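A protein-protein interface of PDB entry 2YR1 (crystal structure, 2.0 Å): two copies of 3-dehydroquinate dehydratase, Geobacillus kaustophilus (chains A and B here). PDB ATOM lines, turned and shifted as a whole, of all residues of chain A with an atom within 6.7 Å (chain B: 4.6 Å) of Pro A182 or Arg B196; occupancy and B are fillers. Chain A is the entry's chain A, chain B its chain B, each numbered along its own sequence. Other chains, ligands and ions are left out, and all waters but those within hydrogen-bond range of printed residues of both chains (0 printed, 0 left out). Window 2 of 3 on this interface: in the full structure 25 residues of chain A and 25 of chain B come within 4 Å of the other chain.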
ATOM      1  N   PRO A 179     -16.448  -7.684  34.738  1.00  0.00           N
ATOM      2  CA  PRO A 179     -17.542  -8.165  33.886  1.00  0.00           C
ATOM      3  C   PRO A 179     -18.816  -8.381  34.697  1.00  0.00           C
ATOM      4  O   PRO A 179     -18.755  -8.736  35.857  1.00  0.00           O
ATOM      5  CB  PRO A 179     -16.981  -9.471  33.329  1.00  0.00           C
ATOM      6  CG  PRO A 179     -16.220 -10.003  34.475  1.00  0.00           C
ATOM      7  CD  PRO A 179     -15.489  -8.769  35.018  1.00  0.00           C
ATOM      8  N   LYS A 180     -19.960  -8.192  34.070  1.00  0.00           N
ATOM      9  CA  LYS A 180     -21.227  -8.386  34.760  1.00  0.00           C
ATOM     10  C   LYS A 180     -21.967  -9.486  34.023  1.00  0.00           C
ATOM     11  O   LYS A 180     -23.079  -9.875  34.392  1.00  0.00           O
ATOM     12  CB  LYS A 180     -22.035  -7.086  34.752  1.00  0.00           C
ATOM     13  CG  LYS A 180     -21.366  -5.933  35.486  1.00  0.00           C
ATOM     14  CD  LYS A 180     -21.045  -6.299  36.921  1.00  0.00           C
ATOM     15  CE  LYS A 180     -20.382  -5.154  37.671  1.00  0.00           C
ATOM     16  NZ  LYS A 180     -21.309  -4.009  37.847  1.00  0.00           N
ATOM     17  N   SER A 181     -21.317 -10.012  32.992  1.00  0.00           N
ATOM     18  CA  SER A 181     -21.893 -11.064  32.167  1.00  0.00           C
ATOM     19  C   SER A 181     -20.811 -11.725  31.307  1.00  0.00           C
ATOM     20  O   SER A 181     -19.727 -11.179  31.139  1.00  0.00           O
ATOM     21  CB  SER A 181     -22.924 -10.464  31.221  1.00  0.00           C
ATOM     22  OG  SER A 181     -22.239  -9.783  30.184  1.00  0.00           O
ATOM     23  N   PRO A 182     -21.098 -12.917  30.761  1.00  0.00           N
ATOM     24  CA  PRO A 182     -20.126 -13.614  29.914  1.00  0.00           C
ATOM     25  C   PRO A 182     -19.809 -12.743  28.702  1.00  0.00           C
ATOM     26  O   PRO A 182     -18.666 -12.690  28.220  1.00  0.00           O
ATOM     27  CB  PRO A 182     -20.862 -14.897  29.538  1.00  0.00           C
ATOM     28  CG  PRO A 182     -21.593 -15.210  30.809  1.00  0.00           C
ATOM     29  CD  PRO A 182     -22.151 -13.844  31.214  1.00  0.00           C
ATOM     30  N   GLU A 183     -20.821 -12.042  28.207  1.00  0.00           N
ATOM     31  CA  GLU A 183     -20.586 -11.181  27.067  1.00  0.00           C
ATOM     32  C   GLU A 183     -19.489 -10.160  27.371  1.00  0.00           C
ATOM     33  O   GLU A 183     -18.676  -9.857  26.500  1.00  0.00           O
ATOM     34  CB  GLU A 183     -21.875 -10.469  26.635  1.00  0.00           C
ATOM     35  CG  GLU A 183     -21.678  -9.634  25.379  1.00  0.00           C
ATOM     36  CD  GLU A 183     -20.889 -10.385  24.303  1.00  0.00           C
ATOM     37  OE1 GLU A 183     -19.921  -9.810  23.729  1.00  0.00           O
ATOM     38  OE2 GLU A 183     -21.240 -11.558  24.039  1.00  0.00           O
ATOM     39  N   ASP A 184     -19.463  -9.641  28.596  1.00  0.00           N
ATOM     40  CA  ASP A 184     -18.440  -8.672  28.999  1.00  0.00           C
ATOM     41  C   ASP A 184     -17.055  -9.286  28.945  1.00  0.00           C
ATOM     42  O   ASP A 184     -16.088  -8.608  28.599  1.00  0.00           O
ATOM     43  CB  ASP A 184     -18.665  -8.168  30.420  1.00  0.00           C
ATOM     44  CG  ASP A 184     -19.744  -7.117  30.506  1.00  0.00           C
ATOM     45  OD1 ASP A 184     -20.041  -6.448  29.477  1.00  0.00           O
ATOM     46  OD2 ASP A 184     -20.276  -6.964  31.622  1.00  0.00           O
ATOM     47  N   VAL A 185     -16.963 -10.558  29.315  1.00  0.00           N
ATOM     48  CA  VAL A 185     -15.679 -11.250  29.293  1.00  0.00           C
ATOM     49  C   VAL A 185     -15.155 -11.324  27.860  1.00  0.00           C
ATOM     50  O   VAL A 185     -13.983 -11.080  27.616  1.00  0.00           O
ATOM     51  CB  VAL A 185     -15.803 -12.676  29.897  1.00  0.00           C
ATOM     52  CG1 VAL A 185     -14.491 -13.396  29.811  1.00  0.00           C
ATOM     53  CG2 VAL A 185     -16.242 -12.574  31.365  1.00  0.00           C
ATOM     54  N   LEU A 186     -16.034 -11.624  26.910  1.00  0.00           N
ATOM     55  CA  LEU A 186     -15.636 -11.706  25.506  1.00  0.00           C
ATOM     56  C   LEU A 186     -15.260 -10.291  24.994  1.00  0.00           C
ATOM     57  O   LEU A 186     -14.354 -10.154  24.197  1.00  0.00           O
ATOM     58  CB  LEU A 186     -16.777 -12.324  24.683  1.00  0.00           C
ATOM     59  CG  LEU A 186     -17.104 -13.795  25.025  1.00  0.00           C
ATOM     60  CD1 LEU A 186     -18.197 -14.302  24.101  1.00  0.00           C
ATOM     61  CD2 LEU A 186     -15.849 -14.675  24.880  1.00  0.00           C
ATOM     62  N   VAL A 187     -15.964  -9.248  25.448  1.00  0.00           N
ATOM     63  CA  VAL A 187     -15.609  -7.876  25.057  1.00  0.00           C
ATOM     64  C   VAL A 187     -14.129  -7.597  25.456  1.00  0.00           C
ATOM     65  O   VAL A 187     -13.324  -7.070  24.664  1.00  0.00           O
ATOM     66  CB  VAL A 187     -16.527  -6.852  25.765  1.00  0.00           C
ATOM     67  CG1 VAL A 187     -15.953  -5.465  25.674  1.00  0.00           C
ATOM     68  CG2 VAL A 187     -17.901  -6.905  25.140  1.00  0.00           C
ATOM     69  N   LEU A 211     -16.304 -14.507  37.036  1.00  0.00           N
ATOM     70  CA  LEU A 211     -16.661 -14.438  35.631  1.00  0.00           C
ATOM     71  C   LEU A 211     -15.418 -14.273  34.775  1.00  0.00           C
ATOM     72  O   LEU A 211     -15.331 -14.833  33.690  1.00  0.00           O
ATOM     73  CB  LEU A 211     -17.588 -13.251  35.416  1.00  0.00           C
ATOM     74  CG  LEU A 211     -18.905 -13.444  34.676  1.00  0.00           C
ATOM     75  CD1 LEU A 211     -19.442 -14.851  34.870  1.00  0.00           C
ATOM     76  CD2 LEU A 211     -19.875 -12.395  35.188  1.00  0.00           C
ATOM     77  N   ASN B   2     -26.776 -22.725  35.080  1.00  0.00           N
ATOM     78  CA  ASN B   2     -26.900 -23.857  34.161  1.00  0.00           C
ATOM     79  C   ASN B   2     -26.312 -23.417  32.835  1.00  0.00           C
ATOM     80  O   ASN B   2     -26.448 -22.258  32.442  1.00  0.00           O
ATOM     81  CB  ASN B   2     -28.360 -24.241  33.962  1.00  0.00           C
ATOM     82  CG  ASN B   2     -28.977 -24.827  35.208  1.00  0.00           C
ATOM     83  OD1 ASN B   2     -28.651 -25.942  35.614  1.00  0.00           O
ATOM     84  ND2 ASN B   2     -29.869 -24.066  35.836  1.00  0.00           N
ATOM     85  N   ILE B   3     -25.656 -24.342  32.147  1.00  0.00           N
ATOM     86  CA  ILE B   3     -25.033 -24.039  30.870  1.00  0.00           C
ATOM     87  C   ILE B   3     -26.069 -23.628  29.824  1.00  0.00           C
ATOM     88  O   ILE B   3     -25.858 -22.663  29.082  1.00  0.00           O
ATOM     89  CB  ILE B   3     -24.188 -25.257  30.400  1.00  0.00           C
ATOM     90  CG1 ILE B   3     -23.068 -25.491  31.431  1.00  0.00           C
ATOM     91  CG2 ILE B   3     -23.602 -25.000  29.012  1.00  0.00           C
ATOM     92  CD1 ILE B   3     -22.284 -26.765  31.288  1.00  0.00           C
ATOM     93  N   PRO B   5     -30.419 -22.856  28.976  1.00  0.00           N
ATOM     94  CA  PRO B   5     -31.640 -22.366  29.637  1.00  0.00           C
ATOM     95  C   PRO B   5     -32.481 -23.542  30.158  1.00  0.00           C
ATOM     96  O   PRO B   5     -32.922 -23.546  31.304  1.00  0.00           O
ATOM     97  CB  PRO B   5     -32.359 -21.595  28.527  1.00  0.00           C
ATOM     98  CG  PRO B   5     -31.220 -21.156  27.613  1.00  0.00           C
ATOM     99  CD  PRO B   5     -30.339 -22.388  27.581  1.00  0.00           C
ATOM    100  N   THR B 192     -21.655 -18.613  20.179  1.00  0.00           N
ATOM    101  CA  THR B 192     -22.173 -19.505  21.197  1.00  0.00           C
ATOM    102  C   THR B 192     -22.885 -18.711  22.310  1.00  0.00           C
ATOM    103  O   THR B 192     -23.992 -19.052  22.724  1.00  0.00           O
ATOM    104  CB  THR B 192     -21.034 -20.368  21.786  1.00  0.00           C
ATOM    105  OG1 THR B 192     -20.324 -21.012  20.709  1.00  0.00           O
ATOM    106  CG2 THR B 192     -21.613 -21.439  22.738  1.00  0.00           C
ATOM    107  N   GLU B 193     -22.260 -17.638  22.778  1.00  0.00           N
ATOM    108  CA  GLU B 193     -22.867 -16.823  23.840  1.00  0.00           C
ATOM    109  C   GLU B 193     -24.213 -16.224  23.401  1.00  0.00           C
ATOM    110  O   GLU B 193     -25.213 -16.300  24.129  1.00  0.00           O
ATOM    111  CB  GLU B 193     -21.902 -15.706  24.259  1.00  0.00           C
ATOM    112  CG  GLU B 193     -22.449 -14.757  25.345  1.00  0.00           C
ATOM    113  CD  GLU B 193     -22.888 -15.491  26.603  1.00  0.00           C
ATOM    114  OE1 GLU B 193     -22.104 -16.326  27.103  1.00  0.00           O
ATOM    115  OE2 GLU B 193     -24.011 -15.237  27.105  1.00  0.00           O
ATOM    116  N   GLU B 194     -24.239 -15.649  22.204  1.00  0.00           N
ATOM    117  CA  GLU B 194     -25.449 -15.038  21.663  1.00  0.00           C
ATOM    118  C   GLU B 194     -26.563 -16.078  21.442  1.00  0.00           C
ATOM    119  O   GLU B 194     -27.724 -15.826  21.761  1.00  0.00           O
ATOM    120  CB  GLU B 194     -25.117 -14.319  20.343  1.00  0.00           C
ATOM    121  CG  GLU B 194     -26.170 -13.326  19.849  1.00  0.00           C
ATOM    122  CD  GLU B 194     -25.662 -12.466  18.690  1.00  0.00           C
ATOM    123  OE1 GLU B 194     -24.446 -12.155  18.655  1.00  0.00           O
ATOM    124  OE2 GLU B 194     -26.479 -12.085  17.819  1.00  0.00           O
ATOM    125  N   ALA B 195     -26.213 -17.238  20.890  1.00  0.00           N
ATOM    126  CA  ALA B 195     -27.195 -18.296  20.638  1.00  0.00           C
ATOM    127  C   ALA B 195     -27.765 -18.839  21.947  1.00  0.00           C
ATOM    128  O   ALA B 195     -28.929 -19.250  22.018  1.00  0.00           O
ATOM    129  CB  ALA B 195     -26.536 -19.455  19.831  1.00  0.00           C
ATOM    130  N   ARG B 196     -26.947 -18.874  22.990  1.00  0.00           N
ATOM    131  CA  ARG B 196     -27.445 -19.396  24.249  1.00  0.00           C
ATOM    132  C   ARG B 196     -28.558 -18.520  24.812  1.00  0.00           C
ATOM    133  O   ARG B 196     -29.427 -19.000  25.530  1.00  0.00           O
ATOM    134  CB  ARG B 196     -26.344 -19.500  25.298  1.00  0.00           C
ATOM    135  CG  ARG B 196     -26.947 -19.622  26.694  1.00  0.00           C
ATOM    136  CD  ARG B 196     -26.000 -20.149  27.724  1.00  0.00           C
ATOM    137  NE  ARG B 196     -24.951 -19.204  28.050  1.00  0.00           N
ATOM    138  CZ  ARG B 196     -24.081 -19.392  29.035  1.00  0.00           C
ATOM    139  NH1 ARG B 196     -24.158 -20.492  29.785  1.00  0.00           N
ATOM    140  NH2 ARG B 196     -23.120 -18.502  29.249  1.00  0.00           N
ATOM    141  N   ARG B 197     -28.517 -17.234  24.496  1.00  0.00           N
ATOM    142  CA  ARG B 197     -29.527 -16.321  25.013  1.00  0.00           C
ATOM    143  C   ARG B 197     -30.770 -16.292  24.150  1.00  0.00           C
ATOM    144  O   ARG B 197     -31.838 -15.901  24.609  1.00  0.00           O
ATOM    145  CB  ARG B 197     -28.946 -14.905  25.153  1.00  0.00           C
ATOM    146  CG  ARG B 197     -27.975 -14.765  26.308  1.00  0.00           C
ATOM    147  CD  ARG B 197     -27.508 -13.336  26.483  1.00  0.00           C
ATOM    148  NE  ARG B 197     -26.579 -13.211  27.602  1.00  0.00           N
ATOM    149  CZ  ARG B 197     -26.907 -13.384  28.881  1.00  0.00           C
ATOM    150  NH1 ARG B 197     -28.154 -13.687  29.217  1.00  0.00           N
ATOM    151  NH2 ARG B 197     -25.982 -13.269  29.832  1.00  0.00           N
ATOM    152  N   GLU B 198     -30.629 -16.748  22.911  1.00  0.00           N
ATOM    153  CA  GLU B 198     -31.726 -16.749  21.963  1.00  0.00           C
ATOM    154  C   GLU B 198     -32.470 -18.071  21.739  1.00  0.00           C
ATOM    155  O   GLU B 198     -33.669 -18.059  21.478  1.00  0.00           O
ATOM    156  CB  GLU B 198     -31.223 -16.224  20.618  1.00  0.00           C
ATOM    157  CG  GLU B 198     -32.194 -16.426  19.478  1.00  0.00           C
ATOM    158  CD  GLU B 198     -31.625 -15.978  18.153  1.00  0.00           C
ATOM    159  OE1 GLU B 198     -32.300 -16.192  17.120  1.00  0.00           O
ATOM    160  OE2 GLU B 198     -30.509 -15.415  18.144  1.00  0.00           O
ATOM    161  N   LEU B 199     -31.782 -19.202  21.834  1.00  0.00           N
ATOM    162  CA  LEU B 199     -32.431 -20.489  21.590  1.00  0.00           C
ATOM    163  C   LEU B 199     -32.868 -21.189  22.875  1.00  0.00           C
ATOM    164  O   LEU B 199     -32.353 -20.893  23.953  1.00  0.00           O
ATOM    165  CB  LEU B 199     -31.492 -21.397  20.780  1.00  0.00           C
ATOM    166  CG  LEU B 199     -30.952 -20.757  19.488  1.00  0.00           C
ATOM    167  CD1 LEU B 199     -29.995 -21.712  18.804  1.00  0.00           C
ATOM    168  CD2 LEU B 199     -32.104 -20.379  18.555  1.00  0.00           C
ATOM    169  N   LEU B 203     -26.667 -26.268  23.335  1.00  0.00           N
ATOM    170  CA  LEU B 203     -25.752 -26.115  22.218  1.00  0.00           C
ATOM    171  C   LEU B 203     -24.456 -26.854  22.422  1.00  0.00           C
ATOM    172  O   LEU B 203     -24.008 -27.019  23.543  1.00  0.00           O
ATOM    173  CB  LEU B 203     -25.391 -24.651  22.055  1.00  0.00           C
ATOM    174  CG  LEU B 203     -26.545 -23.662  21.996  1.00  0.00           C
ATOM    175  CD1 LEU B 203     -25.954 -22.257  22.036  1.00  0.00           C
ATOM    176  CD2 LEU B 203     -27.368 -23.877  20.732  1.00  0.00           C
ATOM    177  N   TRP B 220     -18.013 -24.038  27.715  1.00  0.00           N
ATOM    178  CA  TRP B 220     -19.205 -24.139  28.552  1.00  0.00           C
ATOM    179  C   TRP B 220     -19.525 -22.833  29.279  1.00  0.00           C
ATOM    180  O   TRP B 220     -20.683 -22.556  29.599  1.00  0.00           O
ATOM    181  CB  TRP B 220     -19.061 -25.282  29.557  1.00  0.00           C
ATOM    182  CG  TRP B 220     -17.889 -25.156  30.455  1.00  0.00           C
ATOM    183  CD1 TRP B 220     -16.584 -25.429  30.156  1.00  0.00           C
ATOM    184  CD2 TRP B 220     -17.907 -24.693  31.803  1.00  0.00           C
ATOM    185  NE1 TRP B 220     -15.784 -25.157  31.239  1.00  0.00           N
ATOM    186  CE2 TRP B 220     -16.570 -24.705  32.267  1.00  0.00           C
ATOM    187  CE3 TRP B 220     -18.920 -24.269  32.666  1.00  0.00           C
ATOM    188  CZ2 TRP B 220     -16.221 -24.307  33.565  1.00  0.00           C
ATOM    189  CZ3 TRP B 220     -18.573 -23.869  33.964  1.00  0.00           C
ATOM    190  CH2 TRP B 220     -17.233 -23.893  34.395  1.00  0.00           C
ATOM    191  N   LEU B 221     -18.504 -22.022  29.532  1.00  0.00           N
ATOM    192  CA  LEU B 221     -18.717 -20.746  30.201  1.00  0.00           C
ATOM    193  C   LEU B 221     -19.557 -19.850  29.291  1.00  0.00           C
ATOM    194  O   LEU B 221     -20.105 -18.839  29.736  1.00  0.00           O
ATOM    195  CB  LEU B 221     -17.369 -20.065  30.485  1.00  0.00           C
ATOM    196  CG  LEU B 221     -16.449 -20.758  31.503  1.00  0.00           C
ATOM    197  CD1 LEU B 221     -15.073 -20.130  31.439  1.00  0.00           C
ATOM    198  CD2 LEU B 221     -17.034 -20.629  32.919  1.00  0.00           C
ATOM    199  N   PHE B 222     -19.647 -20.208  28.012  1.00  0.00           N
ATOM    200  CA  PHE B 222     -20.418 -19.397  27.070  1.00  0.00           C
ATOM    201  C   PHE B 222     -21.609 -20.125  26.451  1.00  0.00           C
ATOM    202  O   PHE B 222     -22.209 -19.664  25.478  1.00  0.00           O
ATOM    203  CB  PHE B 222     -19.470 -18.853  25.993  1.00  0.00           C
ATOM    204  CG  PHE B 222     -18.327 -18.073  26.566  1.00  0.00           C
ATOM    205  CD1 PHE B 222     -18.522 -16.778  27.038  1.00  0.00           C
ATOM    206  CD2 PHE B 222     -17.087 -18.662  26.740  1.00  0.00           C
ATOM    207  CE1 PHE B 222     -17.489 -16.088  27.684  1.00  0.00           C
ATOM    208  CE2 PHE B 222     -16.048 -17.988  27.382  1.00  0.00           C
ATOM    209  CZ  PHE B 222     -16.253 -16.699  27.855  1.00  0.00           C
ATOM    210  N   GLY B 223     -21.954 -21.269  27.012  1.00  0.00           N
ATOM    211  CA  GLY B 223     -23.115 -21.982  26.510  1.00  0.00           C
ATOM    212  C   GLY B 223     -22.934 -23.308  25.806  1.00  0.00           C
ATOM    213  O   GLY B 223     -23.944 -23.899  25.421  1.00  0.00           O
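NH1 of Arg B196 sits at hydrogen-bond distance from O of Ile B3 (2.8 Å).
The backbone NH of Glu A183 sits close to the side-chain hydroxyl of Ser A181.
The side-chain carboxylate (OE2) of Glu B193 lies within salt-bridge range of the guanidinium group (NE) of Arg B197, at 3.3 Å.
The backbone carbonyl oxygen of Leu B221 sits at hydrogen-bond distance from the guanidinium group of Arg B196 (3.1 Å).
The backbone NH (N) of Glu B193 sits close to the backbone carbonyl oxygen (O) of Phe B222 (3.4 Å).
OE1 of Glu B193 lies within salt-bridge range of NH2 of Arg B196.
Of the 16 printed residues of chain B, 3 touch a printed residue of chain A.
Printed residues of chain B that touch a printed residue of chain A: Glu B193, Arg B196 and Phe B222.
Printed residues of chain A that touch a printed residue of chain B: Pro A182, Glu A183 and Leu A186.
Among the printed residues, pairs that only touch across the chains: Pro A182 with Glu B193 (3.1 Å), Leu A186 with Phe B222 (3.5 Å), Pro A182 with Phe B222 (3.6 Å), Glu A183 with Glu B193 (3.7 Å), Pro A182 with Arg B196 (3.95 Å) and Leu A186 with Glu B193 (3.97 Å).
Ser A181 touches none of the printed residues of chain B.
Of the printed residues of chain B, Pro A182 touches Glu B193 (3.1 Å), Arg B196 (3.95 Å) and Phe B222 (3.6 Å).
Printed residues of chain B within 4 Å of Glu A183: Glu B193.
Of the printed residues of chain B, Leu A186 touches Glu B193 (3.97 Å) and Phe B222 (3.5 Å).
Printed residues of chain A within 4 Å of Glu B193: Pro A182 (3.1 Å), Glu A183 (3.7 Å) and Leu A186 (3.97 Å).
Arg B196 touches one residue of chain A.
Printed residues of chain A within 4 Å of Phe B222: Pro A182 (3.6 Å) and Leu A186 (3.5 Å).
The nearest printed residue of chain B that does not touch Pro A182 is Leu B221 (4.02 Å).
The nearest printed residue of chain A that does not touch Arg B196 is Glu A183 (6.9 Å).
No position is printed for both chains.
Of the 6 pairs that touch across the chains among the printed residues, none has its exchanged pair printed and touching as well.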
